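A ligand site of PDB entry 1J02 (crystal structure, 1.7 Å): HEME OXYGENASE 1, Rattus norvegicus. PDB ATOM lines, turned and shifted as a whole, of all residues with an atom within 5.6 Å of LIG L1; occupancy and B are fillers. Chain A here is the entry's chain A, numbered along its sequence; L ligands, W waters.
An iron atom (FE1) of LIG L1 is bound by a ring nitrogen (NE2) of His 25, 2.2 Å away.
OH of Tyr 134 lies within hydrogen-bond range of O3 of LIG L1 (2.6 Å).
NZ of Lys 179 is in salt-bridge range of O1 of LIG L1, 2.7 Å away.
An oxygen (O4) of LIG L1 is in salt-bridge range of the guanidinium group of Arg 183 (2.8 Å).
N of Gly 143 sits close to O1 of LG2 L2, 3.1 Å away.
An oxygen (O1) of LG2 L2 is in hydrogen-bond range of the backbone NH (N) of Gly 144 (3.2 Å).
FE1 of LIG L1 is bound by N1 of LG2 L2, 2.1 Å away.
A ring nitrogen (ND1) of His 25 is in hydrogen-bond range of the side-chain carboxylate (OE2) of Glu 29 (2.9 Å).
The side-chain hydroxyl (OH) of Tyr 134 is in hydrogen-bond range of the side-chain hydroxyl (OG1) of Thr 21, at 3.5 Å.
The side-chain amino group (NZ) of Lys 179 lies within hydrogen-bond range of the side-chain hydroxyl (OG) of Ser 142 (2.9 Å).
The guanidinium group (NH1) of Arg 136 lies within hydrogen-bond range of the side-chain amide oxygen (OD1) of Asn 210 (2.9 Å).
O of Met 34 lies close to OE1 of Gln 38, at 3.3 Å.
The backbone carbonyl oxygen (O) of Gly 139 is in hydrogen-bond range of the backbone NH (N) of Gly 144, 3.0 Å away.
The side-chain hydroxyl of Ser 142 sits at hydrogen-bond distance from the backbone carbonyl oxygen of Leu 138, 2.7 Å away.
The side-chain amide oxygen (OE1) of Gln 38 lies close to the backbone carbonyl oxygen (O) of Glu 29 (2.9 Å).
Lys 18 touches LIG L1.
Glu 29 touches LIG L1 (CB to C18, 3.4 Å).
SD of Met 34 touches C19 of LIG L1, 3.4 Å away.
Gln 38 touches LIG L1.
O of Thr 135 touches C31 of LIG L1, at 3.4 Å.
NH1 of Arg 136 touches C26 of LIG L1, 3.1 Å away.
CB of Leu 138 touches C32 of LIG L1, at 3.9 Å.
CA of Gly 139 touches C27 of LIG L1, 3.4 Å away.
Ser 142 touches LIG L1 (OG to C11, 3.4 Å).
Gly 143 touches LIG L1.
Leu 147 touches LIG L1 (CD2 to C19, 3.4 Å).
CE2 of Phe 207 touches C25 of LIG L1 (3.5 Å).
Asn 210 touches LIG L1 (ND2 to C26, 3.5 Å).
Phe 214 touches LIG L1 (CE2 to C24, 3.7 Å).
Hydrophobic or aromatic side chains within 4 Å of LIG L1: His 25, Met 34, Tyr 134, Leu 138, Leu 147, Phe 207 and Phe 214.
Within 4 Å of LIG L1: Lys 18, His 25, Glu 29, Met 34, Gln 38, Tyr 134, Thr 135, Arg 136, Leu 138, Gly 139, Ser 142, Gly 143, Leu 147, Lys 179, Arg 183, Phe 207, Asn 210 and Phe 214.
The nearest printed residue that does not touch LIG L1 is Ala 28 (4.05 Å).
Water W3 lies within hydrogen-bond range of an oxygen (O3) of LIG L1 (2.7 Å), the backbone carbonyl oxygen (O) of Ser 14 (2.9 Å) and the guanidinium group (NE) of Arg 183 (3.2 Å).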
ATOM      1  N   SER A  14      31.852  36.716  19.722  1.00  0.00           N
ATOM      2  CA  SER A  14      30.538  36.126  19.969  1.00  0.00           C
ATOM      3  C   SER A  14      29.430  36.918  19.283  1.00  0.00           C
ATOM      4  O   SER A  14      28.525  36.328  18.678  1.00  0.00           O
ATOM      5  CB  SER A  14      30.247  36.044  21.469  1.00  0.00           C
ATOM      6  OG  SER A  14      30.148  37.330  22.047  1.00  0.00           O
ATOM      7  N   LEU A  17      29.716  36.572  15.415  1.00  0.00           N
ATOM      8  CA  LEU A  17      29.209  35.302  14.935  1.00  0.00           C
ATOM      9  C   LEU A  17      27.682  35.263  14.908  1.00  0.00           C
ATOM     10  O   LEU A  17      27.093  34.782  13.950  1.00  0.00           O
ATOM     11  CB  LEU A  17      29.741  34.149  15.789  1.00  0.00           C
ATOM     12  CG  LEU A  17      31.175  33.703  15.484  1.00  0.00           C
ATOM     13  CD1 LEU A  17      31.669  32.749  16.559  1.00  0.00           C
ATOM     14  CD2 LEU A  17      31.215  33.028  14.127  1.00  0.00           C
ATOM     15  N   LYS A  18      27.053  35.753  15.970  1.00  0.00           N
ATOM     16  CA  LYS A  18      25.595  35.750  16.004  1.00  0.00           C
ATOM     17  C   LYS A  18      25.049  36.611  14.876  1.00  0.00           C
ATOM     18  O   LYS A  18      24.093  36.243  14.187  1.00  0.00           O
ATOM     19  CB  LYS A  18      25.073  36.277  17.347  1.00  0.00           C
ATOM     20  CG  LYS A  18      23.571  36.155  17.501  1.00  0.00           C
ATOM     21  CD  LYS A  18      23.109  36.602  18.874  1.00  0.00           C
ATOM     22  CE  LYS A  18      21.611  36.373  19.045  1.00  0.00           C
ATOM     23  NZ  LYS A  18      21.121  36.794  20.392  1.00  0.00           N
ATOM     24  N   THR A  21      25.624  34.908  11.350  1.00  0.00           N
ATOM     25  CA  THR A  21      24.829  33.722  11.043  1.00  0.00           C
ATOM     26  C   THR A  21      23.331  33.820  11.315  1.00  0.00           C
ATOM     27  O   THR A  21      22.626  32.847  11.124  1.00  0.00           O
ATOM     28  CB  THR A  21      25.370  32.490  11.813  1.00  0.00           C
ATOM     29  OG1 THR A  21      25.212  32.712  13.225  1.00  0.00           O
ATOM     30  CG2 THR A  21      26.847  32.282  11.513  1.00  0.00           C
ATOM     31  N   HIS A  25      20.716  31.173   9.781  1.00  0.00           N
ATOM     32  CA  HIS A  25      20.096  30.327  10.806  1.00  0.00           C
ATOM     33  C   HIS A  25      18.605  30.240  10.527  1.00  0.00           C
ATOM     34  O   HIS A  25      17.992  29.195  10.688  1.00  0.00           O
ATOM     35  CB  HIS A  25      20.332  30.898  12.214  1.00  0.00           C
ATOM     36  CG  HIS A  25      19.687  30.101  13.293  1.00  0.00           C
ATOM     37  ND1 HIS A  25      18.316  30.072  13.487  1.00  0.00           N
ATOM     38  CD2 HIS A  25      20.207  29.266  14.221  1.00  0.00           C
ATOM     39  CE1 HIS A  25      18.031  29.251  14.479  1.00  0.00           C
ATOM     40  NE2 HIS A  25      19.157  28.755  14.950  1.00  0.00           N
ATOM     41  N   ALA A  28      18.142  27.832   7.834  1.00  0.00           N
ATOM     42  CA  ALA A  28      18.401  26.485   8.321  1.00  0.00           C
ATOM     43  C   ALA A  28      17.250  25.914   9.134  1.00  0.00           C
ATOM     44  O   ALA A  28      16.830  24.769   8.919  1.00  0.00           O
ATOM     45  CB  ALA A  28      19.679  26.482   9.173  1.00  0.00           C
ATOM     46  N   GLU A  29      16.719  26.699  10.058  1.00  0.00           N
ATOM     47  CA  GLU A  29      15.631  26.223  10.895  1.00  0.00           C
ATOM     48  C   GLU A  29      14.334  26.071  10.117  1.00  0.00           C
ATOM     49  O   GLU A  29      13.393  25.420  10.576  1.00  0.00           O
ATOM     50  CB  GLU A  29      15.427  27.153  12.095  1.00  0.00           C
ATOM     51  CG  GLU A  29      14.992  28.543  11.755  1.00  0.00           C
ATOM     52  CD  GLU A  29      14.885  29.410  12.997  1.00  0.00           C
ATOM     53  OE1 GLU A  29      14.163  29.005  13.933  1.00  0.00           O
ATOM     54  OE2 GLU A  29      15.524  30.483  13.032  1.00  0.00           O
ATOM     55  N   MET A  34      13.606  20.130   8.793  1.00  0.00           N
ATOM     56  CA  MET A  34      13.428  20.730  10.108  1.00  0.00           C
ATOM     57  C   MET A  34      12.007  21.237  10.288  1.00  0.00           C
ATOM     58  O   MET A  34      11.452  21.172  11.393  1.00  0.00           O
ATOM     59  CB  MET A  34      14.416  21.872  10.318  1.00  0.00           C
ATOM     60  CG  MET A  34      15.834  21.409  10.556  1.00  0.00           C
ATOM     61  SD  MET A  34      15.925  20.399  12.043  1.00  0.00           S
ATOM     62  CE  MET A  34      16.211  18.804  11.366  1.00  0.00           C
ATOM     63  N   GLN A  38       9.764  19.980  13.255  1.00  0.00           N
ATOM     64  CA  GLN A  38       9.112  20.908  14.171  1.00  0.00           C
ATOM     65  C   GLN A  38       7.595  20.749  14.229  1.00  0.00           C
ATOM     66  O   GLN A  38       6.971  21.104  15.225  1.00  0.00           O
ATOM     67  CB  GLN A  38       9.473  22.351  13.796  1.00  0.00           C
ATOM     68  CG  GLN A  38      10.904  22.734  14.132  1.00  0.00           C
ATOM     69  CD  GLN A  38      11.288  24.096  13.590  1.00  0.00           C
ATOM     70  OE1 GLN A  38      11.420  24.285  12.380  1.00  0.00           O
ATOM     71  NE2 GLN A  38      11.460  25.057  14.488  1.00  0.00           N
ATOM     72  N   TYR A 114      30.622  17.309   4.561  1.00  0.00           N
ATOM     73  CA  TYR A 114      30.731  18.031   5.826  1.00  0.00           C
ATOM     74  C   TYR A 114      31.996  17.562   6.544  1.00  0.00           C
ATOM     75  O   TYR A 114      32.815  18.365   6.992  1.00  0.00           O
ATOM     76  CB  TYR A 114      29.496  17.733   6.680  1.00  0.00           C
ATOM     77  CG  TYR A 114      29.188  18.720   7.798  1.00  0.00           C
ATOM     78  CD1 TYR A 114      30.200  19.406   8.464  1.00  0.00           C
ATOM     79  CD2 TYR A 114      27.877  18.901   8.223  1.00  0.00           C
ATOM     80  CE1 TYR A 114      29.916  20.246   9.544  1.00  0.00           C
ATOM     81  CE2 TYR A 114      27.576  19.723   9.305  1.00  0.00           C
ATOM     82  CZ  TYR A 114      28.600  20.392   9.959  1.00  0.00           C
ATOM     83  OH  TYR A 114      28.279  21.184  11.047  1.00  0.00           O
ATOM     84  N   TYR A 134      31.224  26.158  17.405  1.00  0.00           N
ATOM     85  CA  TYR A 134      30.184  27.140  17.711  1.00  0.00           C
ATOM     86  C   TYR A 134      28.860  26.766  17.053  1.00  0.00           C
ATOM     87  O   TYR A 134      27.821  26.692  17.721  1.00  0.00           O
ATOM     88  CB  TYR A 134      30.612  28.524  17.198  1.00  0.00           C
ATOM     89  CG  TYR A 134      29.474  29.510  17.027  1.00  0.00           C
ATOM     90  CD1 TYR A 134      28.928  30.191  18.111  1.00  0.00           C
ATOM     91  CD2 TYR A 134      28.926  29.745  15.759  1.00  0.00           C
ATOM     92  CE1 TYR A 134      27.886  31.100  17.951  1.00  0.00           C
ATOM     93  CE2 TYR A 134      27.889  30.655  15.585  1.00  0.00           C
ATOM     94  CZ  TYR A 134      27.371  31.327  16.671  1.00  0.00           C
ATOM     95  OH  TYR A 134      26.359  32.247  16.483  1.00  0.00           O
ATOM     96  N   THR A 135      28.910  26.526  15.739  1.00  0.00           N
ATOM     97  CA  THR A 135      27.727  26.183  14.964  1.00  0.00           C
ATOM     98  C   THR A 135      27.006  24.954  15.474  1.00  0.00           C
ATOM     99  O   THR A 135      25.775  24.948  15.587  1.00  0.00           O
ATOM    100  CB  THR A 135      28.094  25.992  13.472  1.00  0.00           C
ATOM    101  OG1 THR A 135      28.563  27.240  12.957  1.00  0.00           O
ATOM    102  CG2 THR A 135      26.866  25.527  12.661  1.00  0.00           C
ATOM    103  N   ARG A 136      27.750  23.893  15.776  1.00  0.00           N
ATOM    104  CA  ARG A 136      27.107  22.685  16.245  1.00  0.00           C
ATOM    105  C   ARG A 136      26.735  22.687  17.724  1.00  0.00           C
ATOM    106  O   ARG A 136      25.561  22.549  18.064  1.00  0.00           O
ATOM    107  CB  ARG A 136      27.961  21.448  15.947  1.00  0.00           C
ATOM    108  CG  ARG A 136      27.914  20.934  14.483  1.00  0.00           C
ATOM    109  CD  ARG A 136      26.475  20.769  13.920  1.00  0.00           C
ATOM    110  NE  ARG A 136      25.552  20.087  14.820  1.00  0.00           N
ATOM    111  CZ  ARG A 136      24.268  19.840  14.561  1.00  0.00           C
ATOM    112  NH1 ARG A 136      23.719  20.228  13.420  1.00  0.00           N
ATOM    113  NH2 ARG A 136      23.508  19.264  15.482  1.00  0.00           N
ATOM    114  N   LEU A 138      26.563  25.127  20.196  1.00  0.00           N
ATOM    115  CA  LEU A 138      25.619  26.113  20.718  1.00  0.00           C
ATOM    116  C   LEU A 138      24.208  25.845  20.216  1.00  0.00           C
ATOM    117  O   LEU A 138      23.220  26.145  20.893  1.00  0.00           O
ATOM    118  CB  LEU A 138      26.065  27.541  20.377  1.00  0.00           C
ATOM    119  CG  LEU A 138      27.361  28.002  21.046  1.00  0.00           C
ATOM    120  CD1 LEU A 138      27.382  29.527  21.096  1.00  0.00           C
ATOM    121  CD2 LEU A 138      27.464  27.452  22.467  1.00  0.00           C
ATOM    122  N   GLY A 139      24.099  25.261  19.026  1.00  0.00           N
ATOM    123  CA  GLY A 139      22.785  24.936  18.507  1.00  0.00           C
ATOM    124  C   GLY A 139      22.191  23.775  19.292  1.00  0.00           C
ATOM    125  O   GLY A 139      20.994  23.778  19.602  1.00  0.00           O
ATOM    126  N   SER A 142      20.494  24.837  22.224  1.00  0.00           N
ATOM    127  CA  SER A 142      19.396  25.759  21.995  1.00  0.00           C
ATOM    128  C   SER A 142      18.230  25.047  21.315  1.00  0.00           C
ATOM    129  O   SER A 142      17.432  24.378  21.974  1.00  0.00           O
ATOM    130  CB  SER A 142      19.898  26.928  21.137  1.00  0.00           C
ATOM    131  OG  SER A 142      21.049  27.537  21.716  1.00  0.00           O
ATOM    132  N   GLY A 143      18.135  25.183  20.007  1.00  0.00           N
ATOM    133  CA  GLY A 143      17.060  24.529  19.271  1.00  0.00           C
ATOM    134  C   GLY A 143      17.072  23.026  19.448  1.00  0.00           C
ATOM    135  O   GLY A 143      16.015  22.387  19.469  1.00  0.00           O
ATOM    136  N   GLY A 144      18.259  22.441  19.577  1.00  0.00           N
ATOM    137  CA  GLY A 144      18.362  21.012  19.772  1.00  0.00           C
ATOM    138  C   GLY A 144      17.546  20.532  20.964  1.00  0.00           C
ATOM    139  O   GLY A 144      17.048  19.405  20.971  1.00  0.00           O
ATOM    140  N   VAL A 146      14.689  21.833  21.951  1.00  0.00           N
ATOM    141  CA  VAL A 146      13.282  21.863  21.579  1.00  0.00           C
ATOM    142  C   VAL A 146      13.025  20.618  20.742  1.00  0.00           C
ATOM    143  O   VAL A 146      12.002  19.940  20.905  1.00  0.00           O
ATOM    144  CB  VAL A 146      12.942  23.115  20.770  1.00  0.00           C
ATOM    145  CG1 VAL A 146      11.474  23.069  20.345  1.00  0.00           C
ATOM    146  CG2 VAL A 146      13.228  24.360  21.594  1.00  0.00           C
ATOM    147  N   LEU A 147      13.955  20.307  19.846  1.00  0.00           N
ATOM    148  CA  LEU A 147      13.821  19.136  18.978  1.00  0.00           C
ATOM    149  C   LEU A 147      13.769  17.855  19.801  1.00  0.00           C
ATOM    150  O   LEU A 147      13.070  16.916  19.451  1.00  0.00           O
ATOM    151  CB  LEU A 147      15.007  19.051  18.005  1.00  0.00           C
ATOM    152  CG  LEU A 147      15.130  20.171  16.979  1.00  0.00           C
ATOM    153  CD1 LEU A 147      16.350  19.924  16.104  1.00  0.00           C
ATOM    154  CD2 LEU A 147      13.865  20.246  16.135  1.00  0.00           C
ATOM    155  N   LYS A 179      26.107  28.524  27.834  1.00  0.00           N
ATOM    156  CA  LYS A 179      26.277  29.218  26.568  1.00  0.00           C
ATOM    157  C   LYS A 179      26.890  30.592  26.812  1.00  0.00           C
ATOM    158  O   LYS A 179      27.721  31.057  26.026  1.00  0.00           O
ATOM    159  CB  LYS A 179      24.945  29.338  25.831  1.00  0.00           C
ATOM    160  CG  LYS A 179      24.518  28.042  25.153  1.00  0.00           C
ATOM    161  CD  LYS A 179      23.240  28.213  24.333  1.00  0.00           C
ATOM    162  CE  LYS A 179      22.029  28.444  25.231  1.00  0.00           C
ATOM    163  NZ  LYS A 179      20.784  28.607  24.421  1.00  0.00           N
ATOM    164  N   ARG A 183      30.351  31.794  25.181  1.00  0.00           N
ATOM    165  CA  ARG A 183      30.468  33.007  24.381  1.00  0.00           C
ATOM    166  C   ARG A 183      31.576  33.892  24.948  1.00  0.00           C
ATOM    167  O   ARG A 183      32.386  34.450  24.213  1.00  0.00           O
ATOM    168  CB  ARG A 183      29.146  33.784  24.385  1.00  0.00           C
ATOM    169  CG  ARG A 183      27.999  33.048  23.703  1.00  0.00           C
ATOM    170  CD  ARG A 183      26.795  33.972  23.521  1.00  0.00           C
ATOM    171  NE  ARG A 183      25.643  33.265  22.958  1.00  0.00           N
ATOM    172  CZ  ARG A 183      24.670  32.720  23.672  1.00  0.00           C
ATOM    173  NH1 ARG A 183      24.680  32.802  25.003  1.00  0.00           N
ATOM    174  NH2 ARG A 183      23.683  32.072  23.076  1.00  0.00           N
ATOM    175  N   PHE A 207      26.869  26.430   8.582  1.00  0.00           N
ATOM    176  CA  PHE A 207      25.416  26.421   8.513  1.00  0.00           C
ATOM    177  C   PHE A 207      24.963  25.869   7.163  1.00  0.00           C
ATOM    178  O   PHE A 207      24.024  25.078   7.093  1.00  0.00           O
ATOM    179  CB  PHE A 207      24.838  27.826   8.707  1.00  0.00           C
ATOM    180  CG  PHE A 207      24.505  28.148  10.136  1.00  0.00           C
ATOM    181  CD1 PHE A 207      25.456  28.702  10.991  1.00  0.00           C
ATOM    182  CD2 PHE A 207      23.239  27.883  10.632  1.00  0.00           C
ATOM    183  CE1 PHE A 207      25.137  29.000  12.318  1.00  0.00           C
ATOM    184  CE2 PHE A 207      22.903  28.173  11.946  1.00  0.00           C
ATOM    185  CZ  PHE A 207      23.862  28.730  12.796  1.00  0.00           C
ATOM    186  N   ASN A 210      25.086  22.179   6.930  1.00  0.00           N
ATOM    187  CA  ASN A 210      23.978  21.563   7.634  1.00  0.00           C
ATOM    188  C   ASN A 210      22.733  21.612   6.766  1.00  0.00           C
ATOM    189  O   ASN A 210      22.018  20.618   6.630  1.00  0.00           O
ATOM    190  CB  ASN A 210      23.738  22.258   8.973  1.00  0.00           C
ATOM    191  CG  ASN A 210      24.663  21.757  10.056  1.00  0.00           C
ATOM    192  OD1 ASN A 210      24.423  20.691  10.632  1.00  0.00           O
ATOM    193  ND2 ASN A 210      25.725  22.488  10.324  1.00  0.00           N
ATOM    194  N   PHE A 214      20.463  18.431   5.407  1.00  0.00           N
ATOM    195  CA  PHE A 214      19.026  18.274   5.587  1.00  0.00           C
ATOM    196  C   PHE A 214      18.293  18.160   4.262  1.00  0.00           C
ATOM    197  O   PHE A 214      17.371  17.349   4.123  1.00  0.00           O
ATOM    198  CB  PHE A 214      18.458  19.439   6.410  1.00  0.00           C
ATOM    199  CG  PHE A 214      19.047  19.548   7.778  1.00  0.00           C
ATOM    200  CD1 PHE A 214      19.168  18.419   8.583  1.00  0.00           C
ATOM    201  CD2 PHE A 214      19.485  20.779   8.278  1.00  0.00           C
ATOM    202  CE1 PHE A 214      19.730  18.509   9.867  1.00  0.00           C
ATOM    203  CE2 PHE A 214      20.039  20.876   9.552  1.00  0.00           C
ATOM    204  CZ  PHE A 214      20.159  19.734  10.349  1.00  0.00           C
HETATM  205  C1  LIG L   1      20.583  29.505  18.568  1.00  0.00           C
HETATM  206  C2  LIG L   1      16.254  27.637  17.551  1.00  0.00           C
HETATM  207  C3  LIG L   1      18.260  24.934  14.058  1.00  0.00           C
HETATM  208  C4  LIG L   1      22.611  26.495  15.354  1.00  0.00           C
HETATM  209  C5  LIG L   1      19.217  29.237  18.623  1.00  0.00           C
HETATM  210  C6  LIG L   1      18.281  29.865  19.536  1.00  0.00           C
HETATM  211  C7  LIG L   1      17.072  29.281  19.303  1.00  0.00           C
HETATM  212  C8  LIG L   1      17.262  28.362  18.174  1.00  0.00           C
HETATM  213  C9  LIG L   1      15.765  29.499  20.022  1.00  0.00           C
HETATM  214  C10 LIG L   1      18.625  30.975  20.541  1.00  0.00           C
HETATM  215  C11 LIG L   1      19.379  30.526  21.833  1.00  0.00           C
HETATM  216  C12 LIG L   1      20.057  31.542  22.568  1.00  0.00           C
HETATM  217  O1  LIG L   1      20.874  31.112  23.487  1.00  0.00           O
HETATM  218  O2  LIG L   1      19.916  32.768  22.378  1.00  0.00           O
HETATM  219  C13 LIG L   1      16.438  26.662  16.565  1.00  0.00           C
HETATM  220  C14 LIG L   1      15.386  25.775  16.075  1.00  0.00           C
HETATM  221  C15 LIG L   1      15.900  25.145  14.991  1.00  0.00           C
HETATM  222  C16 LIG L   1      17.327  25.475  14.959  1.00  0.00           C
HETATM  223  C17 LIG L   1      14.025  25.645  16.712  1.00  0.00           C
HETATM  224  C18 LIG L   1      15.191  24.288  13.966  1.00  0.00           C
HETATM  225  C19 LIG L   1      15.230  22.788  14.300  1.00  0.00           C
HETATM  226  C20 LIG L   1      19.617  25.159  14.064  1.00  0.00           C
HETATM  227  C21 LIG L   1      20.561  24.566  13.126  1.00  0.00           C
HETATM  228  C22 LIG L   1      21.768  25.039  13.493  1.00  0.00           C
HETATM  229  C23 LIG L   1      21.589  25.878  14.651  1.00  0.00           C
HETATM  230  C24 LIG L   1      20.180  23.626  12.000  1.00  0.00           C
HETATM  231  C25 LIG L   1      23.124  24.790  12.795  1.00  0.00           C
HETATM  232  C26 LIG L   1      23.666  23.352  13.056  1.00  0.00           C
HETATM  233  C27 LIG L   1      22.445  27.499  16.325  1.00  0.00           C
HETATM  234  C28 LIG L   1      23.543  28.271  16.904  1.00  0.00           C
HETATM  235  C29 LIG L   1      22.972  29.071  17.831  1.00  0.00           C
HETATM  236  C30 LIG L   1      21.521  28.834  17.780  1.00  0.00           C
HETATM  237  C31 LIG L   1      24.970  28.129  16.473  1.00  0.00           C
HETATM  238  C32 LIG L   1      23.609  30.055  18.797  1.00  0.00           C
HETATM  239  C33 LIG L   1      23.601  31.552  18.256  1.00  0.00           C
HETATM  240  C34 LIG L   1      24.264  32.452  19.121  1.00  0.00           C
HETATM  241  O3  LIG L   1      25.270  33.090  18.705  1.00  0.00           O
HETATM  242  O4  LIG L   1      23.861  32.635  20.304  1.00  0.00           O
HETATM  243  N1  LIG L   1      18.586  28.311  17.797  1.00  0.00           N
HETATM  244  N2  LIG L   1      17.646  26.396  15.938  1.00  0.00           N
HETATM  245  N3  LIG L   1      20.262  26.011  14.972  1.00  0.00           N
HETATM  246  N4  LIG L   1      21.227  27.872  16.858  1.00  0.00           N
HETATM  247 FE1  LIG L   1      19.428  27.152  16.385  1.00  0.00          FE
HETATM  248  N1  LG2 L   2      19.637  25.473  17.633  1.00  0.00           N
HETATM  249  O1  LG2 L   2      19.455  24.391  17.305  1.00  0.00           O
HETATM  250  O   HOH W   1      19.086  31.786  16.610  1.00  0.00           O
HETATM  251  O   HOH W   2      23.583  22.804  16.030  1.00  0.00           O
HETATM  252  O   HOH W   3      26.894  34.547  20.272  1.00  0.00           O
